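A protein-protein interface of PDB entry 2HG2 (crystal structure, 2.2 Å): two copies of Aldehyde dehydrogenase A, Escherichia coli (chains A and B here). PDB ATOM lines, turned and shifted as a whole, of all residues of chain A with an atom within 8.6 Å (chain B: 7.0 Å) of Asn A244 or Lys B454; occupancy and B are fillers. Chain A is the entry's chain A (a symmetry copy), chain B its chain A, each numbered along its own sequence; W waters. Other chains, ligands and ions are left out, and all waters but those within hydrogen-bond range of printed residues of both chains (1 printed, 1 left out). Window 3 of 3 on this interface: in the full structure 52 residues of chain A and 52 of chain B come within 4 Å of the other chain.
Among the printed residues, pairs that only touch across the chains: Met A238 with Met B238 (3.99 Å), Ala A241 with Met B238 (3.9 Å), Ala A242 with Glu B235 (3.6 Å), Ala A242 with Met B238 (3.7 Å), Lys A243 with Glu B235 (3.6 Å), Asn A244 with Lys B454 (3.5 Å), Ile A245 with Glu B235 (3.7 Å), Ile A245 with Leu B252 (3.6 Å), Ile A245 with Arg B453 (3.9 Å), Ile A245 with Gly B456 (3.98 Å), Ile A245 with Ile B457 (3.95 Å), Thr A246 with Met B238 (3.2 Å) and Gln A471 with Trp B452 (3.2 Å).
Printed residues of chain B that touch a printed residue of chain A: Glu B235, Met B238, Leu B252, Trp B452, Arg B453, Lys B454, Gly B456 and Ile B457. Hydrophobic or aromatic side chains of chain B within 4 Å of the printed part of chain A: Met B238, Leu B252, Trp B452 and Ile B457. Of the 20 printed residues of chain A, 8 touch a printed residue of chain B. Along chain A the printed residues that touch a printed residue of chain B span positions 238 to 471.
Met A238 touches its own counterpart, Met B238. Of the 13 pairs that touch across the chains among the printed residues, 1 has its exchanged pair printed and touching as well.
Asn A244 touches just one residue of chain B: Lys B454. Of the printed residues of chain B, Lys A243 touches Glu B235 (3.6 Å). Of the printed residues of chain A, Met B238 touches Met A238, Ala A241, Ala A242 and Thr A246. Of the printed residues of chain B, Ala A242 touches Glu B235 (3.6 Å) and Met B238 (3.7 Å). Of the printed residues of chain B, Ala A241 touches Met B238 (3.9 Å). Printed residues of chain B within 4 Å of Ile A245: Glu B235, Leu B252, Arg B453, Gly B456 and Ile B457. The nearest residue of chain B that does not touch Asn A244 is Arg B453 (5.0 Å). The nearest residue of chain A that does not touch Lys B454 is Ile A245 (4.1 Å). The nearest printed residue of chain B that does not touch Thr A246 is Ile B457 (4.03 Å).
Water W1 bridges the side-chain amide oxygen (OE1) of Gln A471 and the backbone NH (N) of Arg B453.
The backbone carbonyl oxygen (O) of Asp B408 sits at hydrogen-bond distance from the backbone NH (N) of Lys B454 (2.8 Å). The backbone carbonyl oxygen (O) of Tyr B409 is in hydrogen-bond range of the guanidinium group (NH2) of Arg B453, at 2.8 Å. The backbone NH (N) of Leu B252 is in hydrogen-bond range of the backbone carbonyl oxygen (O) of Ser B455. The backbone carbonyl oxygen (O) of Gly B410 sits at hydrogen-bond distance from the backbone NH (N) of Trp B452 (2.7 Å). The backbone NH (N) of Thr A246 sits at hydrogen-bond distance from the backbone carbonyl oxygen (O) of Ala A241 (3.0 Å). ND2 of Asn A244 lies within hydrogen-bond range of O of Gly A218, at 2.8 Å.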
ATOM      1  N   GLN A 214       9.442   9.430  17.462  1.00  0.00           N
ATOM      2  CA  GLN A 214      10.765   9.421  18.063  1.00  0.00           C
ATOM      3  C   GLN A 214      11.853   9.912  17.120  1.00  0.00           C
ATOM      4  O   GLN A 214      12.798  10.572  17.552  1.00  0.00           O
ATOM      5  CB  GLN A 214      11.104   8.020  18.556  1.00  0.00           C
ATOM      6  CG  GLN A 214      10.345   7.618  19.805  1.00  0.00           C
ATOM      7  CD  GLN A 214      10.685   8.505  20.990  1.00  0.00           C
ATOM      8  OE1 GLN A 214       9.908   9.387  21.377  1.00  0.00           O
ATOM      9  NE2 GLN A 214      11.863   8.281  21.568  1.00  0.00           N
ATOM     10  N   GLU A 215      11.730   9.595  15.835  1.00  0.00           N
ATOM     11  CA  GLU A 215      12.736  10.026  14.867  1.00  0.00           C
ATOM     12  C   GLU A 215      12.652  11.544  14.685  1.00  0.00           C
ATOM     13  O   GLU A 215      13.665  12.219  14.464  1.00  0.00           O
ATOM     14  CB  GLU A 215      12.516   9.310  13.527  1.00  0.00           C
ATOM     15  CG  GLU A 215      13.501   9.679  12.419  1.00  0.00           C
ATOM     16  CD  GLU A 215      14.955   9.400  12.783  1.00  0.00           C
ATOM     17  OE1 GLU A 215      15.210   8.413  13.501  1.00  0.00           O
ATOM     18  OE2 GLU A 215      15.845  10.161  12.341  1.00  0.00           O
ATOM     19  N   ALA A 217      11.984  13.610  16.964  1.00  0.00           N
ATOM     20  CA  ALA A 217      12.541  14.245  18.151  1.00  0.00           C
ATOM     21  C   ALA A 217      14.032  13.957  18.336  1.00  0.00           C
ATOM     22  O   ALA A 217      14.737  14.732  18.982  1.00  0.00           O
ATOM     23  CB  ALA A 217      11.768  13.786  19.403  1.00  0.00           C
ATOM     24  N   GLY A 218      14.513  12.862  17.752  1.00  0.00           N
ATOM     25  CA  GLY A 218      15.903  12.489  17.939  1.00  0.00           C
ATOM     26  C   GLY A 218      16.853  12.571  16.770  1.00  0.00           C
ATOM     27  O   GLY A 218      18.016  12.194  16.897  1.00  0.00           O
ATOM     28  N   ASN A 219      16.383  13.055  15.630  1.00  0.00           N
ATOM     29  CA  ASN A 219      17.253  13.167  14.471  1.00  0.00           C
ATOM     30  C   ASN A 219      18.114  14.417  14.656  1.00  0.00           C
ATOM     31  O   ASN A 219      17.597  15.511  14.861  1.00  0.00           O
ATOM     32  CB  ASN A 219      16.411  13.263  13.199  1.00  0.00           C
ATOM     33  CG  ASN A 219      17.252  13.323  11.953  1.00  0.00           C
ATOM     34  OD1 ASN A 219      18.024  14.259  11.759  1.00  0.00           O
ATOM     35  ND2 ASN A 219      17.106  12.323  11.095  1.00  0.00           N
ATOM     36  N   PRO A 220      19.446  14.268  14.574  1.00  0.00           N
ATOM     37  CA  PRO A 220      20.382  15.382  14.743  1.00  0.00           C
ATOM     38  C   PRO A 220      20.191  16.600  13.847  1.00  0.00           C
ATOM     39  O   PRO A 220      20.713  17.668  14.149  1.00  0.00           O
ATOM     40  CB  PRO A 220      21.752  14.718  14.551  1.00  0.00           C
ATOM     41  CG  PRO A 220      21.460  13.579  13.624  1.00  0.00           C
ATOM     42  CD  PRO A 220      20.159  13.037  14.174  1.00  0.00           C
ATOM     43  N   LYS A 221      19.449  16.464  12.756  1.00  0.00           N
ATOM     44  CA  LYS A 221      19.238  17.605  11.866  1.00  0.00           C
ATOM     45  C   LYS A 221      18.070  18.487  12.304  1.00  0.00           C
ATOM     46  O   LYS A 221      17.862  19.567  11.752  1.00  0.00           O
ATOM     47  CB  LYS A 221      18.998  17.132  10.430  1.00  0.00           C
ATOM     48  CG  LYS A 221      20.202  16.477   9.788  1.00  0.00           C
ATOM     49  CD  LYS A 221      19.838  15.910   8.437  1.00  0.00           C
ATOM     50  CE  LYS A 221      21.055  15.308   7.758  1.00  0.00           C
ATOM     51  NZ  LYS A 221      20.697  14.791   6.421  1.00  0.00           N
ATOM     52  N   VAL A 222      17.306  18.024  13.287  1.00  0.00           N
ATOM     53  CA  VAL A 222      16.171  18.790  13.781  1.00  0.00           C
ATOM     54  C   VAL A 222      16.660  19.843  14.781  1.00  0.00           C
ATOM     55  O   VAL A 222      17.351  19.524  15.746  1.00  0.00           O
ATOM     56  CB  VAL A 222      15.118  17.854  14.446  1.00  0.00           C
ATOM     57  CG1 VAL A 222      14.012  18.679  15.107  1.00  0.00           C
ATOM     58  CG2 VAL A 222      14.523  16.919  13.391  1.00  0.00           C
ATOM     59  N   ALA A 223      16.324  21.102  14.529  1.00  0.00           N
ATOM     60  CA  ALA A 223      16.742  22.185  15.409  1.00  0.00           C
ATOM     61  C   ALA A 223      15.773  22.292  16.586  1.00  0.00           C
ATOM     62  O   ALA A 223      16.156  22.690  17.694  1.00  0.00           O
ATOM     63  CB  ALA A 223      16.792  23.492  14.638  1.00  0.00           C
ATOM     64  N   MET A 238      11.185  14.737  25.355  1.00  0.00           N
ATOM     65  CA  MET A 238      12.285  15.528  25.884  1.00  0.00           C
ATOM     66  C   MET A 238      13.509  14.642  26.130  1.00  0.00           C
ATOM     67  O   MET A 238      14.640  15.050  25.883  1.00  0.00           O
ATOM     68  CB  MET A 238      11.862  16.232  27.177  1.00  0.00           C
ATOM     69  CG  MET A 238      12.603  17.540  27.409  1.00  0.00           C
ATOM     70  SD  MET A 238      12.075  18.441  28.889  1.00  0.00           S
ATOM     71  CE  MET A 238      13.692  18.896  29.573  1.00  0.00           C
ATOM     72  N   ALA A 239      13.278  13.422  26.605  1.00  0.00           N
ATOM     73  CA  ALA A 239      14.374  12.496  26.861  1.00  0.00           C
ATOM     74  C   ALA A 239      15.114  12.200  25.553  1.00  0.00           C
ATOM     75  O   ALA A 239      16.347  12.172  25.516  1.00  0.00           O
ATOM     76  CB  ALA A 239      13.833  11.198  27.470  1.00  0.00           C
ATOM     77  N   THR A 240      14.353  11.983  24.483  1.00  0.00           N
ATOM     78  CA  THR A 240      14.927  11.694  23.167  1.00  0.00           C
ATOM     79  C   THR A 240      15.697  12.893  22.620  1.00  0.00           C
ATOM     80  O   THR A 240      16.789  12.744  22.072  1.00  0.00           O
ATOM     81  CB  THR A 240      13.825  11.316  22.171  1.00  0.00           C
ATOM     82  OG1 THR A 240      13.150  10.147  22.645  1.00  0.00           O
ATOM     83  CG2 THR A 240      14.412  11.045  20.792  1.00  0.00           C
ATOM     84  N   ALA A 241      15.124  14.080  22.773  1.00  0.00           N
ATOM     85  CA  ALA A 241      15.752  15.308  22.309  1.00  0.00           C
ATOM     86  C   ALA A 241      17.071  15.558  23.042  1.00  0.00           C
ATOM     87  O   ALA A 241      18.006  16.118  22.477  1.00  0.00           O
ATOM     88  CB  ALA A 241      14.805  16.486  22.530  1.00  0.00           C
ATOM     89  N   ALA A 242      17.129  15.136  24.301  1.00  0.00           N
ATOM     90  CA  ALA A 242      18.308  15.307  25.141  1.00  0.00           C
ATOM     91  C   ALA A 242      19.580  14.801  24.482  1.00  0.00           C
ATOM     92  O   ALA A 242      20.653  15.388  24.654  1.00  0.00           O
ATOM     93  CB  ALA A 242      18.103  14.586  26.478  1.00  0.00           C
ATOM     94  N   LYS A 243      19.454  13.715  23.726  1.00  0.00           N
ATOM     95  CA  LYS A 243      20.592  13.098  23.050  1.00  0.00           C
ATOM     96  C   LYS A 243      21.373  14.016  22.128  1.00  0.00           C
ATOM     97  O   LYS A 243      22.588  13.896  22.019  1.00  0.00           O
ATOM     98  CB  LYS A 243      20.126  11.867  22.269  1.00  0.00           C
ATOM     99  CG  LYS A 243      19.623  10.757  23.173  1.00  0.00           C
ATOM    100  CD  LYS A 243      18.753   9.763  22.426  1.00  0.00           C
ATOM    101  CE  LYS A 243      18.038   8.833  23.407  1.00  0.00           C
ATOM    102  NZ  LYS A 243      16.985   8.012  22.736  1.00  0.00           N
ATOM    103  N   ASN A 244      20.687  14.938  21.470  1.00  0.00           N
ATOM    104  CA  ASN A 244      21.361  15.846  20.551  1.00  0.00           C
ATOM    105  C   ASN A 244      21.199  17.305  20.955  1.00  0.00           C
ATOM    106  O   ASN A 244      21.431  18.212  20.153  1.00  0.00           O
ATOM    107  CB  ASN A 244      20.826  15.633  19.134  1.00  0.00           C
ATOM    108  CG  ASN A 244      21.164  14.258  18.591  1.00  0.00           C
ATOM    109  OD1 ASN A 244      22.335  13.903  18.451  1.00  0.00           O
ATOM    110  ND2 ASN A 244      20.140  13.478  18.284  1.00  0.00           N
ATOM    111  N   ILE A 245      20.813  17.521  22.209  1.00  0.00           N
ATOM    112  CA  ILE A 245      20.604  18.868  22.727  1.00  0.00           C
ATOM    113  C   ILE A 245      19.622  19.602  21.815  1.00  0.00           C
ATOM    114  O   ILE A 245      19.790  20.782  21.501  1.00  0.00           O
ATOM    115  CB  ILE A 245      21.927  19.678  22.795  1.00  0.00           C
ATOM    116  CG1 ILE A 245      23.062  18.809  23.340  1.00  0.00           C
ATOM    117  CG2 ILE A 245      21.739  20.881  23.716  1.00  0.00           C
ATOM    118  CD1 ILE A 245      22.799  18.259  24.746  1.00  0.00           C
ATOM    119  N   THR A 246      18.597  18.880  21.379  1.00  0.00           N
ATOM    120  CA  THR A 246      17.575  19.448  20.513  1.00  0.00           C
ATOM    121  C   THR A 246      16.606  20.278  21.352  1.00  0.00           C
ATOM    122  O   THR A 246      16.181  19.862  22.430  1.00  0.00           O
ATOM    123  CB  THR A 246      16.807  18.334  19.781  1.00  0.00           C
ATOM    124  OG1 THR A 246      17.731  17.557  19.004  1.00  0.00           O
ATOM    125  CG2 THR A 246      15.752  18.926  18.859  1.00  0.00           C
ATOM    126  N   LYS A 247      16.268  21.461  20.862  1.00  0.00           N
ATOM    127  CA  LYS A 247      15.352  22.339  21.578  1.00  0.00           C
ATOM    128  C   LYS A 247      13.940  21.750  21.549  1.00  0.00           C
ATOM    129  O   LYS A 247      13.552  21.104  20.573  1.00  0.00           O
ATOM    130  CB  LYS A 247      15.358  23.735  20.925  1.00  0.00           C
ATOM    131  CG  LYS A 247      14.460  24.750  21.615  1.00  0.00           C
ATOM    132  CD  LYS A 247      14.362  26.083  20.857  1.00  0.00           C
ATOM    133  CE  LYS A 247      13.470  27.058  21.637  1.00  0.00           C
ATOM    134  NZ  LYS A 247      13.203  28.363  20.957  1.00  0.00           N
ATOM    135  N   GLN A 471      16.160  32.343  16.714  1.00  0.00           N
ATOM    136  CA  GLN A 471      17.293  32.272  17.616  1.00  0.00           C
ATOM    137  C   GLN A 471      18.144  33.478  17.258  1.00  0.00           C
ATOM    138  O   GLN A 471      18.056  34.005  16.145  1.00  0.00           O
ATOM    139  CB  GLN A 471      18.067  30.956  17.451  1.00  0.00           C
ATOM    140  CG  GLN A 471      18.749  30.762  16.118  1.00  0.00           C
ATOM    141  CD  GLN A 471      19.291  29.359  15.970  1.00  0.00           C
ATOM    142  OE1 GLN A 471      19.525  28.664  16.963  1.00  0.00           O
ATOM    143  NE2 GLN A 471      19.500  28.931  14.731  1.00  0.00           N
ATOM    144  N   SER B 230      30.379  20.313  29.472  1.00  0.00           N
ATOM    145  CA  SER B 230      30.557  19.603  28.207  1.00  0.00           C
ATOM    146  C   SER B 230      29.229  19.116  27.654  1.00  0.00           C
ATOM    147  O   SER B 230      28.260  18.965  28.389  1.00  0.00           O
ATOM    148  CB  SER B 230      31.484  18.400  28.391  1.00  0.00           C
ATOM    149  OG  SER B 230      30.855  17.393  29.162  1.00  0.00           O
ATOM    150  N   VAL B 231      29.194  18.864  26.352  1.00  0.00           N
ATOM    151  CA  VAL B 231      27.983  18.391  25.702  1.00  0.00           C
ATOM    152  C   VAL B 231      27.541  17.085  26.356  1.00  0.00           C
ATOM    153  O   VAL B 231      26.351  16.859  26.578  1.00  0.00           O
ATOM    154  CB  VAL B 231      28.223  18.159  24.193  1.00  0.00           C
ATOM    155  CG1 VAL B 231      29.331  17.140  23.999  1.00  0.00           C
ATOM    156  CG2 VAL B 231      26.942  17.686  23.524  1.00  0.00           C
ATOM    157  N   GLU B 235      23.881  16.467  28.072  1.00  0.00           N
ATOM    158  CA  GLU B 235      22.938  15.428  27.683  1.00  0.00           C
ATOM    159  C   GLU B 235      22.341  14.760  28.916  1.00  0.00           C
ATOM    160  O   GLU B 235      21.129  14.566  29.000  1.00  0.00           O
ATOM    161  CB  GLU B 235      23.639  14.368  26.829  1.00  0.00           C
ATOM    162  CG  GLU B 235      24.130  14.864  25.481  1.00  0.00           C
ATOM    163  CD  GLU B 235      24.976  13.825  24.756  1.00  0.00           C
ATOM    164  OE1 GLU B 235      24.574  12.638  24.739  1.00  0.00           O
ATOM    165  OE2 GLU B 235      26.036  14.197  24.202  1.00  0.00           O
ATOM    166  N   MET B 238      19.817  17.149  30.601  1.00  0.00           N
ATOM    167  CA  MET B 238      18.549  17.316  29.908  1.00  0.00           C
ATOM    168  C   MET B 238      17.703  16.046  30.031  1.00  0.00           C
ATOM    169  O   MET B 238      16.489  16.114  30.196  1.00  0.00           O
ATOM    170  CB  MET B 238      18.788  17.663  28.435  1.00  0.00           C
ATOM    171  CG  MET B 238      17.670  18.502  27.835  1.00  0.00           C
ATOM    172  SD  MET B 238      17.953  18.997  26.116  1.00  0.00           S
ATOM    173  CE  MET B 238      16.318  18.644  25.415  1.00  0.00           C
ATOM    174  N   LEU B 250      21.300  25.506  28.991  1.00  0.00           N
ATOM    175  CA  LEU B 250      22.603  24.883  28.830  1.00  0.00           C
ATOM    176  C   LEU B 250      23.555  25.652  27.917  1.00  0.00           C
ATOM    177  O   LEU B 250      23.151  26.208  26.902  1.00  0.00           O
ATOM    178  CB  LEU B 250      22.407  23.462  28.289  1.00  0.00           C
ATOM    179  CG  LEU B 250      21.351  22.612  29.015  1.00  0.00           C
ATOM    180  CD1 LEU B 250      21.082  21.319  28.248  1.00  0.00           C
ATOM    181  CD2 LEU B 250      21.829  22.315  30.433  1.00  0.00           C
ATOM    182  N   GLU B 251      24.823  25.683  28.306  1.00  0.00           N
ATOM    183  CA  GLU B 251      25.879  26.327  27.535  1.00  0.00           C
ATOM    184  C   GLU B 251      26.922  25.217  27.526  1.00  0.00           C
ATOM    185  O   GLU B 251      27.548  24.940  28.550  1.00  0.00           O
ATOM    186  CB  GLU B 251      26.393  27.560  28.274  1.00  0.00           C
ATOM    187  CG  GLU B 251      27.108  28.563  27.385  1.00  0.00           C
ATOM    188  CD  GLU B 251      28.609  28.364  27.340  1.00  0.00           C
ATOM    189  OE1 GLU B 251      29.337  29.311  27.726  1.00  0.00           O
ATOM    190  OE2 GLU B 251      29.064  27.274  26.921  1.00  0.00           O
ATOM    191  N   LEU B 252      27.104  24.571  26.379  1.00  0.00           N
ATOM    192  CA  LEU B 252      28.023  23.440  26.319  1.00  0.00           C
ATOM    193  C   LEU B 252      29.317  23.608  25.518  1.00  0.00           C
ATOM    194  O   LEU B 252      29.855  22.640  24.992  1.00  0.00           O
ATOM    195  CB  LEU B 252      27.247  22.199  25.836  1.00  0.00           C
ATOM    196  CG  LEU B 252      25.878  21.983  26.517  1.00  0.00           C
ATOM    197  CD1 LEU B 252      25.156  20.780  25.923  1.00  0.00           C
ATOM    198  CD2 LEU B 252      26.068  21.798  28.027  1.00  0.00           C
ATOM    199  N   GLY B 253      29.824  24.831  25.437  1.00  0.00           N
ATOM    200  CA  GLY B 253      31.074  25.067  24.732  1.00  0.00           C
ATOM    201  C   GLY B 253      31.038  24.911  23.224  1.00  0.00           C
ATOM    202  O   GLY B 253      29.964  24.887  22.616  1.00  0.00           O
ATOM    203  N   SER B 407      29.916  21.873  11.789  1.00  0.00           N
ATOM    204  CA  SER B 407      30.203  21.549  13.185  1.00  0.00           C
ATOM    205  C   SER B 407      28.912  21.357  13.988  1.00  0.00           C
ATOM    206  O   SER B 407      27.874  21.916  13.640  1.00  0.00           O
ATOM    207  CB  SER B 407      31.022  22.699  13.797  1.00  0.00           C
ATOM    208  OG  SER B 407      31.221  22.552  15.195  1.00  0.00           O
ATOM    209  N   ASP B 408      28.976  20.572  15.061  1.00  0.00           N
ATOM    210  CA  ASP B 408      27.803  20.356  15.906  1.00  0.00           C
ATOM    211  C   ASP B 408      27.688  21.459  16.942  1.00  0.00           C
ATOM    212  O   ASP B 408      26.725  21.506  17.706  1.00  0.00           O
ATOM    213  CB  ASP B 408      27.871  19.015  16.632  1.00  0.00           C
ATOM    214  CG  ASP B 408      27.670  17.846  15.705  1.00  0.00           C
ATOM    215  OD1 ASP B 408      26.770  17.920  14.842  1.00  0.00           O
ATOM    216  OD2 ASP B 408      28.404  16.850  15.849  1.00  0.00           O
ATOM    217  N   TYR B 409      28.692  22.328  16.974  1.00  0.00           N
ATOM    218  CA  TYR B 409      28.705  23.446  17.904  1.00  0.00           C
ATOM    219  C   TYR B 409      28.419  24.736  17.135  1.00  0.00           C
ATOM    220  O   TYR B 409      28.775  24.859  15.953  1.00  0.00           O
ATOM    221  CB  TYR B 409      30.057  23.536  18.620  1.00  0.00           C
ATOM    222  CG  TYR B 409      30.435  22.283  19.390  1.00  0.00           C
ATOM    223  CD1 TYR B 409      31.297  21.332  18.839  1.00  0.00           C
ATOM    224  CD2 TYR B 409      29.913  22.037  20.663  1.00  0.00           C
ATOM    225  CE1 TYR B 409      31.632  20.162  19.537  1.00  0.00           C
ATOM    226  CE2 TYR B 409      30.238  20.873  21.369  1.00  0.00           C
ATOM    227  CZ  TYR B 409      31.099  19.942  20.804  1.00  0.00           C
ATOM    228  OH  TYR B 409      31.443  18.807  21.519  1.00  0.00           O
ATOM    229  N   GLY B 410      27.770  25.689  17.803  1.00  0.00           N
ATOM    230  CA  GLY B 410      27.426  26.943  17.157  1.00  0.00           C
ATOM    231  C   GLY B 410      27.288  28.119  18.103  1.00  0.00           C
ATOM    232  O   GLY B 410      26.305  28.863  18.055  1.00  0.00           O
ATOM    233  N   GLY B 451      24.260  29.562  22.434  1.00  0.00           N
ATOM    234  CA  GLY B 451      24.734  28.710  21.358  1.00  0.00           C
ATOM    235  C   GLY B 451      23.718  27.988  20.499  1.00  0.00           C
ATOM    236  O   GLY B 451      22.655  27.578  20.955  1.00  0.00           O
ATOM    237  N   TRP B 452      24.070  27.843  19.229  1.00  0.00           N
ATOM    238  CA  TRP B 452      23.245  27.146  18.260  1.00  0.00           C
ATOM    239  C   TRP B 452      23.597  25.660  18.321  1.00  0.00           C
ATOM    240  O   TRP B 452      24.628  25.278  18.883  1.00  0.00           O
ATOM    241  CB  TRP B 452      23.540  27.680  16.860  1.00  0.00           C
ATOM    242  CG  TRP B 452      22.998  29.061  16.572  1.00  0.00           C
ATOM    243  CD1 TRP B 452      22.794  30.075  17.465  1.00  0.00           C
ATOM    244  CD2 TRP B 452      22.608  29.571  15.290  1.00  0.00           C
ATOM    245  NE1 TRP B 452      22.297  31.185  16.817  1.00  0.00           N
ATOM    246  CE2 TRP B 452      22.174  30.902  15.482  1.00  0.00           C
ATOM    247  CE3 TRP B 452      22.578  29.028  13.997  1.00  0.00           C
ATOM    248  CZ2 TRP B 452      21.717  31.701  14.429  1.00  0.00           C
ATOM    249  CZ3 TRP B 452      22.122  29.828  12.947  1.00  0.00           C
ATOM    250  CH2 TRP B 452      21.698  31.150  13.174  1.00  0.00           C
ATOM    251  N   ARG B 453      22.739  24.829  17.738  1.00  0.00           N
ATOM    252  CA  ARG B 453      22.947  23.389  17.691  1.00  0.00           C
ATOM    253  C   ARG B 453      23.312  22.794  19.054  1.00  0.00           C
ATOM    254  O   ARG B 453      22.633  23.066  20.042  1.00  0.00           O
ATOM    255  CB  ARG B 453      24.006  23.059  16.628  1.00  0.00           C
ATOM    256  CG  ARG B 453      23.577  23.491  15.216  1.00  0.00           C
ATOM    257  CD  ARG B 453      24.608  23.128  14.134  1.00  0.00           C
ATOM    258  NE  ARG B 453      25.844  23.906  14.221  1.00  0.00           N
ATOM    259  CZ  ARG B 453      25.967  25.175  13.837  1.00  0.00           C
ATOM    260  NH1 ARG B 453      24.928  25.827  13.335  1.00  0.00           N
ATOM    261  NH2 ARG B 453      27.137  25.795  13.949  1.00  0.00           N
ATOM    262  N   LYS B 454      24.371  21.996  19.124  1.00  0.00           N
ATOM    263  CA  LYS B 454      24.737  21.375  20.397  1.00  0.00           C
ATOM    264  C   LYS B 454      25.444  22.279  21.409  1.00  0.00           C
ATOM    265  O   LYS B 454      25.764  21.844  22.513  1.00  0.00           O
ATOM    266  CB  LYS B 454      25.578  20.116  20.155  1.00  0.00           C
ATOM    267  CG  LYS B 454      24.846  19.037  19.381  1.00  0.00           C
ATOM    268  CD  LYS B 454      25.613  17.718  19.383  1.00  0.00           C
ATOM    269  CE  LYS B 454      24.926  16.697  18.494  1.00  0.00           C
ATOM    270  NZ  LYS B 454      25.555  15.350  18.581  1.00  0.00           N
ATOM    271  N   SER B 455      25.679  23.534  21.047  1.00  0.00           N
ATOM    272  CA  SER B 455      26.332  24.456  21.964  1.00  0.00           C
ATOM    273  C   SER B 455      25.420  24.869  23.122  1.00  0.00           C
ATOM    274  O   SER B 455      25.890  25.449  24.100  1.00  0.00           O
ATOM    275  CB  SER B 455      26.831  25.694  21.213  1.00  0.00           C
ATOM    276  OG  SER B 455      27.948  25.358  20.405  1.00  0.00           O
ATOM    277  N   GLY B 456      24.124  24.584  23.020  1.00  0.00           N
ATOM    278  CA  GLY B 456      23.239  24.933  24.122  1.00  0.00           C
ATOM    279  C   GLY B 456      21.742  25.062  23.889  1.00  0.00           C
ATOM    280  O   GLY B 456      21.211  24.728  22.827  1.00  0.00           O
ATOM    281  N   ILE B 457      21.063  25.529  24.930  1.00  0.00           N
ATOM    282  CA  ILE B 457      19.625  25.777  24.921  1.00  0.00           C
ATOM    283  C   ILE B 457      19.448  27.011  25.792  1.00  0.00           C
ATOM    284  O   ILE B 457      19.968  27.070  26.905  1.00  0.00           O
ATOM    285  CB  ILE B 457      18.826  24.585  25.509  1.00  0.00           C
ATOM    286  CG1 ILE B 457      18.808  23.441  24.490  1.00  0.00           C
ATOM    287  CG2 ILE B 457      17.382  25.015  25.845  1.00  0.00           C
ATOM    288  CD1 ILE B 457      18.236  22.164  25.023  1.00  0.00           C
HETATM  289  O   HOH W   1      20.035  25.807  17.170  1.00  0.00           O
